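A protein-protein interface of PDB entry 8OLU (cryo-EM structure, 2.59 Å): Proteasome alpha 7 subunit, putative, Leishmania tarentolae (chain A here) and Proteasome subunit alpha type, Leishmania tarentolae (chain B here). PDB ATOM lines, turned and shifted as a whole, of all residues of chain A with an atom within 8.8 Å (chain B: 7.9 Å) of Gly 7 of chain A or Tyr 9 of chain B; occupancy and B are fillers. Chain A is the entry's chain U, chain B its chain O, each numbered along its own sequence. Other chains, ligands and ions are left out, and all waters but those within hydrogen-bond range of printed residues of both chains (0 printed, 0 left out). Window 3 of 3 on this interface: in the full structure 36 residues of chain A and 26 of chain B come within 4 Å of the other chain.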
ATOM      1  N   GLY A   7     -25.431  31.350 -23.789  1.00  0.00           N
ATOM      2  CA  GLY A   7     -24.628  30.814 -22.664  1.00  0.00           C
ATOM      3  C   GLY A   7     -23.132  30.697 -22.986  1.00  0.00           C
ATOM      4  O   GLY A   7     -22.341  30.284 -22.135  1.00  0.00           O
ATOM      5  N   HIS A   8     -22.754  31.107 -24.204  1.00  0.00           N
ATOM      6  CA  HIS A   8     -21.378  31.077 -24.687  1.00  0.00           C
ATOM      7  C   HIS A   8     -20.517  32.192 -24.085  1.00  0.00           C
ATOM      8  O   HIS A   8     -19.339  32.231 -24.415  1.00  0.00           O
ATOM      9  CB  HIS A   8     -21.358  31.177 -26.234  1.00  0.00           C
ATOM     10  CG  HIS A   8     -22.153  32.318 -26.817  1.00  0.00           C
ATOM     11  ND1 HIS A   8     -23.515  32.492 -26.629  1.00  0.00           N
ATOM     12  CD2 HIS A   8     -21.731  33.374 -27.580  1.00  0.00           C
ATOM     13  CE1 HIS A   8     -23.913  33.608 -27.242  1.00  0.00           C
ATOM     14  NE2 HIS A   8     -22.816  34.176 -27.837  1.00  0.00           N
ATOM     15  N   ASP A   9     -21.087  33.133 -23.290  1.00  0.00           N
ATOM     16  CA  ASP A   9     -20.428  34.409 -23.062  1.00  0.00           C
ATOM     17  C   ASP A   9     -20.489  34.853 -21.614  1.00  0.00           C
ATOM     18  O   ASP A   9     -20.296  36.009 -21.285  1.00  0.00           O
ATOM     19  CB  ASP A   9     -20.994  35.513 -23.955  1.00  0.00           C
ATOM     20  CG  ASP A   9     -22.412  35.958 -23.654  1.00  0.00           C
ATOM     21  OD1 ASP A   9     -22.848  36.877 -24.357  1.00  0.00           O
ATOM     22  OD2 ASP A   9     -23.073  35.405 -22.710  1.00  0.00           O
ATOM     23  N   GLN A  10     -20.726  33.923 -20.732  1.00  0.00           N
ATOM     24  CA  GLN A  10     -20.985  34.256 -19.361  1.00  0.00           C
ATOM     25  C   GLN A  10     -19.725  34.068 -18.520  1.00  0.00           C
ATOM     26  O   GLN A  10     -19.605  34.599 -17.405  1.00  0.00           O
ATOM     27  CB  GLN A  10     -22.049  33.290 -18.900  1.00  0.00           C
ATOM     28  CG  GLN A  10     -23.382  33.503 -19.584  1.00  0.00           C
ATOM     29  CD  GLN A  10     -24.170  34.579 -18.894  1.00  0.00           C
ATOM     30  OE1 GLN A  10     -24.462  34.476 -17.698  1.00  0.00           O
ATOM     31  NE2 GLN A  10     -24.470  35.623 -19.652  1.00  0.00           N
ATOM     32  N   SER A  11     -18.809  33.248 -19.029  1.00  0.00           N
ATOM     33  CA  SER A  11     -17.613  32.984 -18.285  1.00  0.00           C
ATOM     34  C   SER A  11     -16.429  33.049 -19.218  1.00  0.00           C
ATOM     35  O   SER A  11     -16.511  32.775 -20.407  1.00  0.00           O
ATOM     36  CB  SER A  11     -17.728  31.657 -17.635  1.00  0.00           C
ATOM     37  OG  SER A  11     -16.828  31.540 -16.521  1.00  0.00           O
ATOM     38  N   THR A  12     -15.332  33.531 -18.677  1.00  0.00           N
ATOM     39  CA  THR A  12     -14.155  33.645 -19.500  1.00  0.00           C
ATOM     40  C   THR A  12     -13.544  32.276 -19.719  1.00  0.00           C
ATOM     41  O   THR A  12     -12.718  32.165 -20.596  1.00  0.00           O
ATOM     42  CB  THR A  12     -13.096  34.515 -18.861  1.00  0.00           C
ATOM     43  OG1 THR A  12     -11.992  34.636 -19.755  1.00  0.00           O
ATOM     44  CG2 THR A  12     -12.561  33.893 -17.591  1.00  0.00           C
ATOM     45  N   ASP A  13     -13.976  31.238 -18.989  1.00  0.00           N
ATOM     46  CA  ASP A  13     -13.459  29.894 -19.201  1.00  0.00           C
ATOM     47  C   ASP A  13     -13.978  29.243 -20.464  1.00  0.00           C
ATOM     48  O   ASP A  13     -13.753  28.083 -20.709  1.00  0.00           O
ATOM     49  CB  ASP A  13     -13.769  28.919 -18.057  1.00  0.00           C
ATOM     50  CG  ASP A  13     -15.224  28.465 -17.917  1.00  0.00           C
ATOM     51  OD1 ASP A  13     -15.468  27.187 -17.901  1.00  0.00           O
ATOM     52  OD2 ASP A  13     -16.117  29.367 -17.765  1.00  0.00           O
ATOM     53  N   VAL A  14     -14.611  29.978 -21.330  1.00  0.00           N
ATOM     54  CA  VAL A  14     -15.315  29.316 -22.395  1.00  0.00           C
ATOM     55  C   VAL A  14     -14.986  29.941 -23.718  1.00  0.00           C
ATOM     56  O   VAL A  14     -15.108  31.142 -23.875  1.00  0.00           O
ATOM     57  CB  VAL A  14     -16.803  29.477 -22.115  1.00  0.00           C
ATOM     58  CG1 VAL A  14     -17.629  29.147 -23.331  1.00  0.00           C
ATOM     59  CG2 VAL A  14     -17.154  28.558 -20.961  1.00  0.00           C
ATOM     60  N   PHE A  15     -14.736  29.110 -24.703  1.00  0.00           N
ATOM     61  CA  PHE A  15     -14.644  29.617 -26.047  1.00  0.00           C
ATOM     62  C   PHE A  15     -15.998  29.627 -26.692  1.00  0.00           C
ATOM     63  O   PHE A  15     -16.795  28.748 -26.488  1.00  0.00           O
ATOM     64  CB  PHE A  15     -13.760  28.755 -26.905  1.00  0.00           C
ATOM     65  CG  PHE A  15     -12.308  28.916 -26.617  1.00  0.00           C
ATOM     66  CD1 PHE A  15     -11.612  30.019 -27.091  1.00  0.00           C
ATOM     67  CD2 PHE A  15     -11.625  27.928 -25.915  1.00  0.00           C
ATOM     68  CE1 PHE A  15     -10.255  30.139 -26.875  1.00  0.00           C
ATOM     69  CE2 PHE A  15     -10.248  28.046 -25.710  1.00  0.00           C
ATOM     70  CZ  PHE A  15      -9.570  29.154 -26.183  1.00  0.00           C
ATOM     71  N   SER A  16     -16.190  30.616 -27.540  1.00  0.00           N
ATOM     72  CA  SER A  16     -17.303  30.603 -28.454  1.00  0.00           C
ATOM     73  C   SER A  16     -16.961  29.639 -29.558  1.00  0.00           C
ATOM     74  O   SER A  16     -15.799  29.276 -29.663  1.00  0.00           O
ATOM     75  CB  SER A  16     -17.506  31.941 -29.045  1.00  0.00           C
ATOM     76  OG  SER A  16     -16.406  32.247 -29.902  1.00  0.00           O
ATOM     77  N   ALA A  17     -17.921  29.380 -30.446  1.00  0.00           N
ATOM     78  CA  ALA A  17     -17.634  28.538 -31.593  1.00  0.00           C
ATOM     79  C   ALA A  17     -16.612  29.132 -32.545  1.00  0.00           C
ATOM     80  O   ALA A  17     -16.093  28.392 -33.355  1.00  0.00           O
ATOM     81  CB  ALA A  17     -18.878  28.239 -32.348  1.00  0.00           C
ATOM     82  N   PHE A  22     -15.607  35.681 -25.190  1.00  0.00           N
ATOM     83  CA  PHE A  22     -16.385  36.878 -25.130  1.00  0.00           C
ATOM     84  C   PHE A  22     -16.172  37.661 -23.865  1.00  0.00           C
ATOM     85  O   PHE A  22     -16.106  38.863 -23.893  1.00  0.00           O
ATOM     86  CB  PHE A  22     -17.826  36.475 -25.307  1.00  0.00           C
ATOM     87  CG  PHE A  22     -18.214  36.428 -26.751  1.00  0.00           C
ATOM     88  CD1 PHE A  22     -18.439  37.595 -27.447  1.00  0.00           C
ATOM     89  CD2 PHE A  22     -18.318  35.237 -27.418  1.00  0.00           C
ATOM     90  CE1 PHE A  22     -18.795  37.568 -28.785  1.00  0.00           C
ATOM     91  CE2 PHE A  22     -18.722  35.210 -28.744  1.00  0.00           C
ATOM     92  CZ  PHE A  22     -18.931  36.370 -29.427  1.00  0.00           C
ATOM     93  N   GLN A  23     -16.105  37.026 -22.721  1.00  0.00           N
ATOM     94  CA  GLN A  23     -15.928  37.813 -21.525  1.00  0.00           C
ATOM     95  C   GLN A  23     -14.681  38.664 -21.585  1.00  0.00           C
ATOM     96  O   GLN A  23     -14.596  39.695 -20.929  1.00  0.00           O
ATOM     97  CB  GLN A  23     -15.813  36.923 -20.322  1.00  0.00           C
ATOM     98  CG  GLN A  23     -17.201  36.459 -19.900  1.00  0.00           C
ATOM     99  CD  GLN A  23     -17.951  37.550 -19.241  1.00  0.00           C
ATOM    100  OE1 GLN A  23     -17.473  38.078 -18.248  1.00  0.00           O
ATOM    101  NE2 GLN A  23     -19.120  37.859 -19.767  1.00  0.00           N
ATOM    102  N   PHE A 127     -13.131  29.728 -14.502  1.00  0.00           N
ATOM    103  CA  PHE A 127     -14.524  30.136 -14.473  1.00  0.00           C
ATOM    104  C   PHE A 127     -14.798  31.047 -13.288  1.00  0.00           C
ATOM    105  O   PHE A 127     -15.741  31.828 -13.282  1.00  0.00           O
ATOM    106  CB  PHE A 127     -15.412  28.902 -14.367  1.00  0.00           C
ATOM    107  CG  PHE A 127     -15.271  28.234 -13.044  1.00  0.00           C
ATOM    108  CD1 PHE A 127     -16.129  28.547 -12.006  1.00  0.00           C
ATOM    109  CD2 PHE A 127     -14.245  27.349 -12.805  1.00  0.00           C
ATOM    110  CE1 PHE A 127     -15.951  28.005 -10.743  1.00  0.00           C
ATOM    111  CE2 PHE A 127     -14.066  26.804 -11.550  1.00  0.00           C
ATOM    112  CZ  PHE A 127     -14.913  27.154 -10.518  1.00  0.00           C
ATOM    113  N   PHE B   6     -25.333  22.685 -23.473  1.00  0.00           N
ATOM    114  CA  PHE B   6     -24.848  22.311 -22.116  1.00  0.00           C
ATOM    115  C   PHE B   6     -23.461  21.685 -22.192  1.00  0.00           C
ATOM    116  O   PHE B   6     -22.652  21.850 -21.286  1.00  0.00           O
ATOM    117  CB  PHE B   6     -25.815  21.341 -21.433  1.00  0.00           C
ATOM    118  CG  PHE B   6     -25.491  21.046 -19.983  1.00  0.00           C
ATOM    119  CD1 PHE B   6     -26.168  21.701 -18.955  1.00  0.00           C
ATOM    120  CD2 PHE B   6     -24.530  20.095 -19.641  1.00  0.00           C
ATOM    121  CE1 PHE B   6     -25.883  21.425 -17.625  1.00  0.00           C
ATOM    122  CE2 PHE B   6     -24.244  19.818 -18.310  1.00  0.00           C
ATOM    123  CZ  PHE B   6     -24.924  20.482 -17.305  1.00  0.00           C
ATOM    124  N   ASP B   7     -23.217  20.944 -23.276  1.00  0.00           N
ATOM    125  CA  ASP B   7     -21.933  20.312 -23.560  1.00  0.00           C
ATOM    126  C   ASP B   7     -21.024  21.260 -24.328  1.00  0.00           C
ATOM    127  O   ASP B   7     -19.867  20.937 -24.533  1.00  0.00           O
ATOM    128  CB  ASP B   7     -22.111  19.005 -24.358  1.00  0.00           C
ATOM    129  CG  ASP B   7     -22.960  19.096 -25.621  1.00  0.00           C
ATOM    130  OD1 ASP B   7     -23.124  20.197 -26.136  1.00  0.00           O
ATOM    131  OD2 ASP B   7     -23.482  18.054 -26.075  1.00  0.00           O
ATOM    132  N   LYS B   8     -21.546  22.391 -24.811  1.00  0.00           N
ATOM    133  CA  LYS B   8     -20.775  23.249 -25.696  1.00  0.00           C
ATOM    134  C   LYS B   8     -19.865  24.146 -24.861  1.00  0.00           C
ATOM    135  O   LYS B   8     -18.870  24.657 -25.365  1.00  0.00           O
ATOM    136  CB  LYS B   8     -21.687  24.051 -26.623  1.00  0.00           C
ATOM    137  CG  LYS B   8     -22.364  23.242 -27.720  1.00  0.00           C
ATOM    138  CD  LYS B   8     -23.362  24.056 -28.539  1.00  0.00           C
ATOM    139  CE  LYS B   8     -24.222  23.203 -29.452  1.00  0.00           C
ATOM    140  NZ  LYS B   8     -23.402  22.269 -30.264  1.00  0.00           N
ATOM    141  N   TYR B   9     -20.180  24.245 -23.573  1.00  0.00           N
ATOM    142  CA  TYR B   9     -19.602  25.228 -22.695  1.00  0.00           C
ATOM    143  C   TYR B   9     -18.816  24.565 -21.573  1.00  0.00           C
ATOM    144  O   TYR B   9     -18.215  25.228 -20.741  1.00  0.00           O
ATOM    145  CB  TYR B   9     -20.687  26.111 -22.077  1.00  0.00           C
ATOM    146  CG  TYR B   9     -21.834  26.518 -22.969  1.00  0.00           C
ATOM    147  CD1 TYR B   9     -21.625  27.084 -24.231  1.00  0.00           C
ATOM    148  CD2 TYR B   9     -23.145  26.316 -22.532  1.00  0.00           C
ATOM    149  CE1 TYR B   9     -22.705  27.440 -25.033  1.00  0.00           C
ATOM    150  CE2 TYR B   9     -24.230  26.666 -23.321  1.00  0.00           C
ATOM    151  CZ  TYR B   9     -24.006  27.236 -24.568  1.00  0.00           C
ATOM    152  OH  TYR B   9     -25.117  27.575 -25.308  1.00  0.00           O
ATOM    153  N   ILE B  10     -18.789  23.257 -21.516  1.00  0.00           N
ATOM    154  CA  ILE B  10     -17.985  22.682 -20.472  1.00  0.00           C
ATOM    155  C   ILE B  10     -17.292  21.457 -21.045  1.00  0.00           C
ATOM    156  O   ILE B  10     -17.586  21.003 -22.135  1.00  0.00           O
ATOM    157  CB  ILE B  10     -18.861  22.443 -19.215  1.00  0.00           C
ATOM    158  CG1 ILE B  10     -18.050  22.482 -17.915  1.00  0.00           C
ATOM    159  CG2 ILE B  10     -19.729  21.193 -19.317  1.00  0.00           C
ATOM    160  CD1 ILE B  10     -18.608  21.577 -16.813  1.00  0.00           C
ATOM    161  N   THR B  11     -16.309  20.969 -20.330  1.00  0.00           N
ATOM    162  CA  THR B  11     -15.483  19.945 -20.891  1.00  0.00           C
ATOM    163  C   THR B  11     -16.111  18.587 -20.572  1.00  0.00           C
ATOM    164  O   THR B  11     -15.590  17.786 -19.814  1.00  0.00           O
ATOM    165  CB  THR B  11     -14.055  20.191 -20.392  1.00  0.00           C
ATOM    166  OG1 THR B  11     -13.135  19.829 -21.439  1.00  0.00           O
ATOM    167  CG2 THR B  11     -13.819  19.499 -19.050  1.00  0.00           C
ATOM    168  N   VAL B  12     -17.263  18.338 -21.163  1.00  0.00           N
ATOM    169  CA  VAL B  12     -17.894  17.034 -21.147  1.00  0.00           C
ATOM    170  C   VAL B  12     -18.071  16.643 -22.589  1.00  0.00           C
ATOM    171  O   VAL B  12     -17.998  17.497 -23.455  1.00  0.00           O
ATOM    172  CB  VAL B  12     -19.275  17.074 -20.491  1.00  0.00           C
ATOM    173  CG1 VAL B  12     -19.147  17.464 -19.040  1.00  0.00           C
ATOM    174  CG2 VAL B  12     -20.199  18.012 -21.231  1.00  0.00           C
ATOM    175  N   TYR B  20     -16.519  19.845 -27.451  1.00  0.00           N
ATOM    176  CA  TYR B  20     -16.717  21.077 -28.162  1.00  0.00           C
ATOM    177  C   TYR B  20     -15.657  22.058 -27.765  1.00  0.00           C
ATOM    178  O   TYR B  20     -15.045  22.614 -28.629  1.00  0.00           O
ATOM    179  CB  TYR B  20     -18.155  21.569 -28.011  1.00  0.00           C
ATOM    180  CG  TYR B  20     -19.060  20.873 -28.990  1.00  0.00           C
ATOM    181  CD1 TYR B  20     -18.754  20.858 -30.338  1.00  0.00           C
ATOM    182  CD2 TYR B  20     -20.195  20.209 -28.589  1.00  0.00           C
ATOM    183  CE1 TYR B  20     -19.551  20.196 -31.260  1.00  0.00           C
ATOM    184  CE2 TYR B  20     -21.034  19.589 -29.501  1.00  0.00           C
ATOM    185  CZ  TYR B  20     -20.694  19.548 -30.837  1.00  0.00           C
ATOM    186  OH  TYR B  20     -21.500  18.917 -31.739  1.00  0.00           O
ATOM    187  N   GLN B  21     -15.412  22.250 -26.490  1.00  0.00           N
ATOM    188  CA  GLN B  21     -14.553  23.336 -26.082  1.00  0.00           C
ATOM    189  C   GLN B  21     -13.175  23.084 -26.643  1.00  0.00           C
ATOM    190  O   GLN B  21     -12.538  24.021 -27.084  1.00  0.00           O
ATOM    191  CB  GLN B  21     -14.521  23.536 -24.574  1.00  0.00           C
ATOM    192  CG  GLN B  21     -15.728  24.313 -24.067  1.00  0.00           C
ATOM    193  CD  GLN B  21     -15.681  25.729 -24.576  1.00  0.00           C
ATOM    194  OE1 GLN B  21     -14.675  26.391 -24.382  1.00  0.00           O
ATOM    195  NE2 GLN B  21     -16.685  26.169 -25.312  1.00  0.00           N
ATOM    196  N   TYR B  24     -13.346  24.187 -30.349  1.00  0.00           N
ATOM    197  CA  TYR B  24     -13.375  25.624 -30.425  1.00  0.00           C
ATOM    198  C   TYR B  24     -12.020  26.219 -30.065  1.00  0.00           C
ATOM    199  O   TYR B  24     -11.555  27.179 -30.652  1.00  0.00           O
ATOM    200  CB  TYR B  24     -14.411  26.144 -29.425  1.00  0.00           C
ATOM    201  CG  TYR B  24     -15.845  25.783 -29.751  1.00  0.00           C
ATOM    202  CD1 TYR B  24     -16.205  25.132 -30.914  1.00  0.00           C
ATOM    203  CD2 TYR B  24     -16.837  26.047 -28.847  1.00  0.00           C
ATOM    204  CE1 TYR B  24     -17.510  24.791 -31.189  1.00  0.00           C
ATOM    205  CE2 TYR B  24     -18.157  25.744 -29.128  1.00  0.00           C
ATOM    206  CZ  TYR B  24     -18.500  25.104 -30.291  1.00  0.00           C
ATOM    207  OH  TYR B  24     -19.833  24.839 -30.471  1.00  0.00           O
ATOM    208  N   ALA B 126     -13.082  20.445 -15.412  1.00  0.00           N
ATOM    209  CA  ALA B 126     -13.989  21.490 -15.879  1.00  0.00           C
ATOM    210  C   ALA B 126     -13.611  22.887 -15.408  1.00  0.00           C
ATOM    211  O   ALA B 126     -13.064  23.092 -14.322  1.00  0.00           O
ATOM    212  CB  ALA B 126     -15.378  21.223 -15.390  1.00  0.00           C
ATOM    213  N   GLY B 127     -13.932  23.863 -16.247  1.00  0.00           N
ATOM    214  CA  GLY B 127     -13.797  25.238 -15.803  1.00  0.00           C
ATOM    215  C   GLY B 127     -12.370  25.771 -15.918  1.00  0.00           C
ATOM    216  O   GLY B 127     -12.076  26.849 -15.420  1.00  0.00           O
ATOM    217  N   LEU B 128     -11.514  25.061 -16.629  1.00  0.00           N
ATOM    218  CA  LEU B 128     -10.262  25.625 -17.066  1.00  0.00           C
ATOM    219  C   LEU B 128     -10.318  25.754 -18.555  1.00  0.00           C
ATOM    220  O   LEU B 128     -10.716  24.799 -19.195  1.00  0.00           O
ATOM    221  CB  LEU B 128      -9.191  24.633 -16.687  1.00  0.00           C
ATOM    222  CG  LEU B 128      -9.017  24.539 -15.184  1.00  0.00           C
ATOM    223  CD1 LEU B 128      -8.019  23.421 -14.848  1.00  0.00           C
ATOM    224  CD2 LEU B 128      -8.591  25.910 -14.642  1.00  0.00           C
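OE1 of Gln 21 of chain B sits at hydrogen-bond distance from N of Phe 15 of chain A. The backbone NH (N) of Phe 127 of chain A is in hydrogen-bond range of the backbone carbonyl oxygen (O) of Gly 127 of chain B.
OG of Ser 11 of chain A sits at hydrogen-bond distance from OD2 of Asp 13 of chain A, 2.6 Å away. The side-chain hydroxyl (OG) of Ser 11 of chain A lies close to the backbone carbonyl oxygen (O) of Phe 127 of chain A, at 3.4 Å. The backbone carbonyl oxygen (O) of Lys 8 of chain B is in hydrogen-bond range of the side-chain amide nitrogen (NE2) of Gln 21 of chain B, 2.7 Å away.
Gly 7 of chain A touches Tyr 9 of chain B (C to CE1, 3.9 Å). His 8 of chain A touches Tyr 9 of chain B (N to CE1, 3.8 Å). Gly 127 of chain B touches Asp 13 of chain A (CA to OD1, 3.3 Å). Tyr 9 of chain B touches Val 14 of chain A. CA of Val 14 of chain A touches OE1 of Gln 21 of chain B, 3.6 Å away. O of Phe 15 of chain A touches CD2 of Tyr 24 of chain B, 3.6 Å away. Ser 16 of chain A touches Tyr 24 of chain B. Tyr 24 of chain B touches Ala 17 of chain A.
Of chain B, only Tyr 9 (3.9 Å) comes within 4 Å of Gly 7 of chain A. Printed residues of chain A within 4 Å of Tyr 9 of chain B: Gly 7, His 8 and Val 14. Printed residues of chain B within 4 Å of His 8 of chain A: Tyr 9. Of the printed residues of chain B, Ala 17 of chain A touches Tyr 24. The nearest residue of chain A that does not touch Tyr 9 of chain B is Asp 13 of chain A (4.4 Å). The nearest printed residue of chain B that does not touch His 8 of chain A is Gln 21 of chain B (6.7 Å).
Hydrophobic or aromatic side chains of chain B that line the printed part of chain A: Tyr 9 and Tyr 24. Of the 14 printed residues of chain A, 8 touch a printed residue of chain B. Hydrophobic or aromatic side chains of chain A that line the printed part of chain B: Val 14, Phe 15, Ala 17 and Phe 127. Among the printed residues, 10 pairs touch across the chains.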
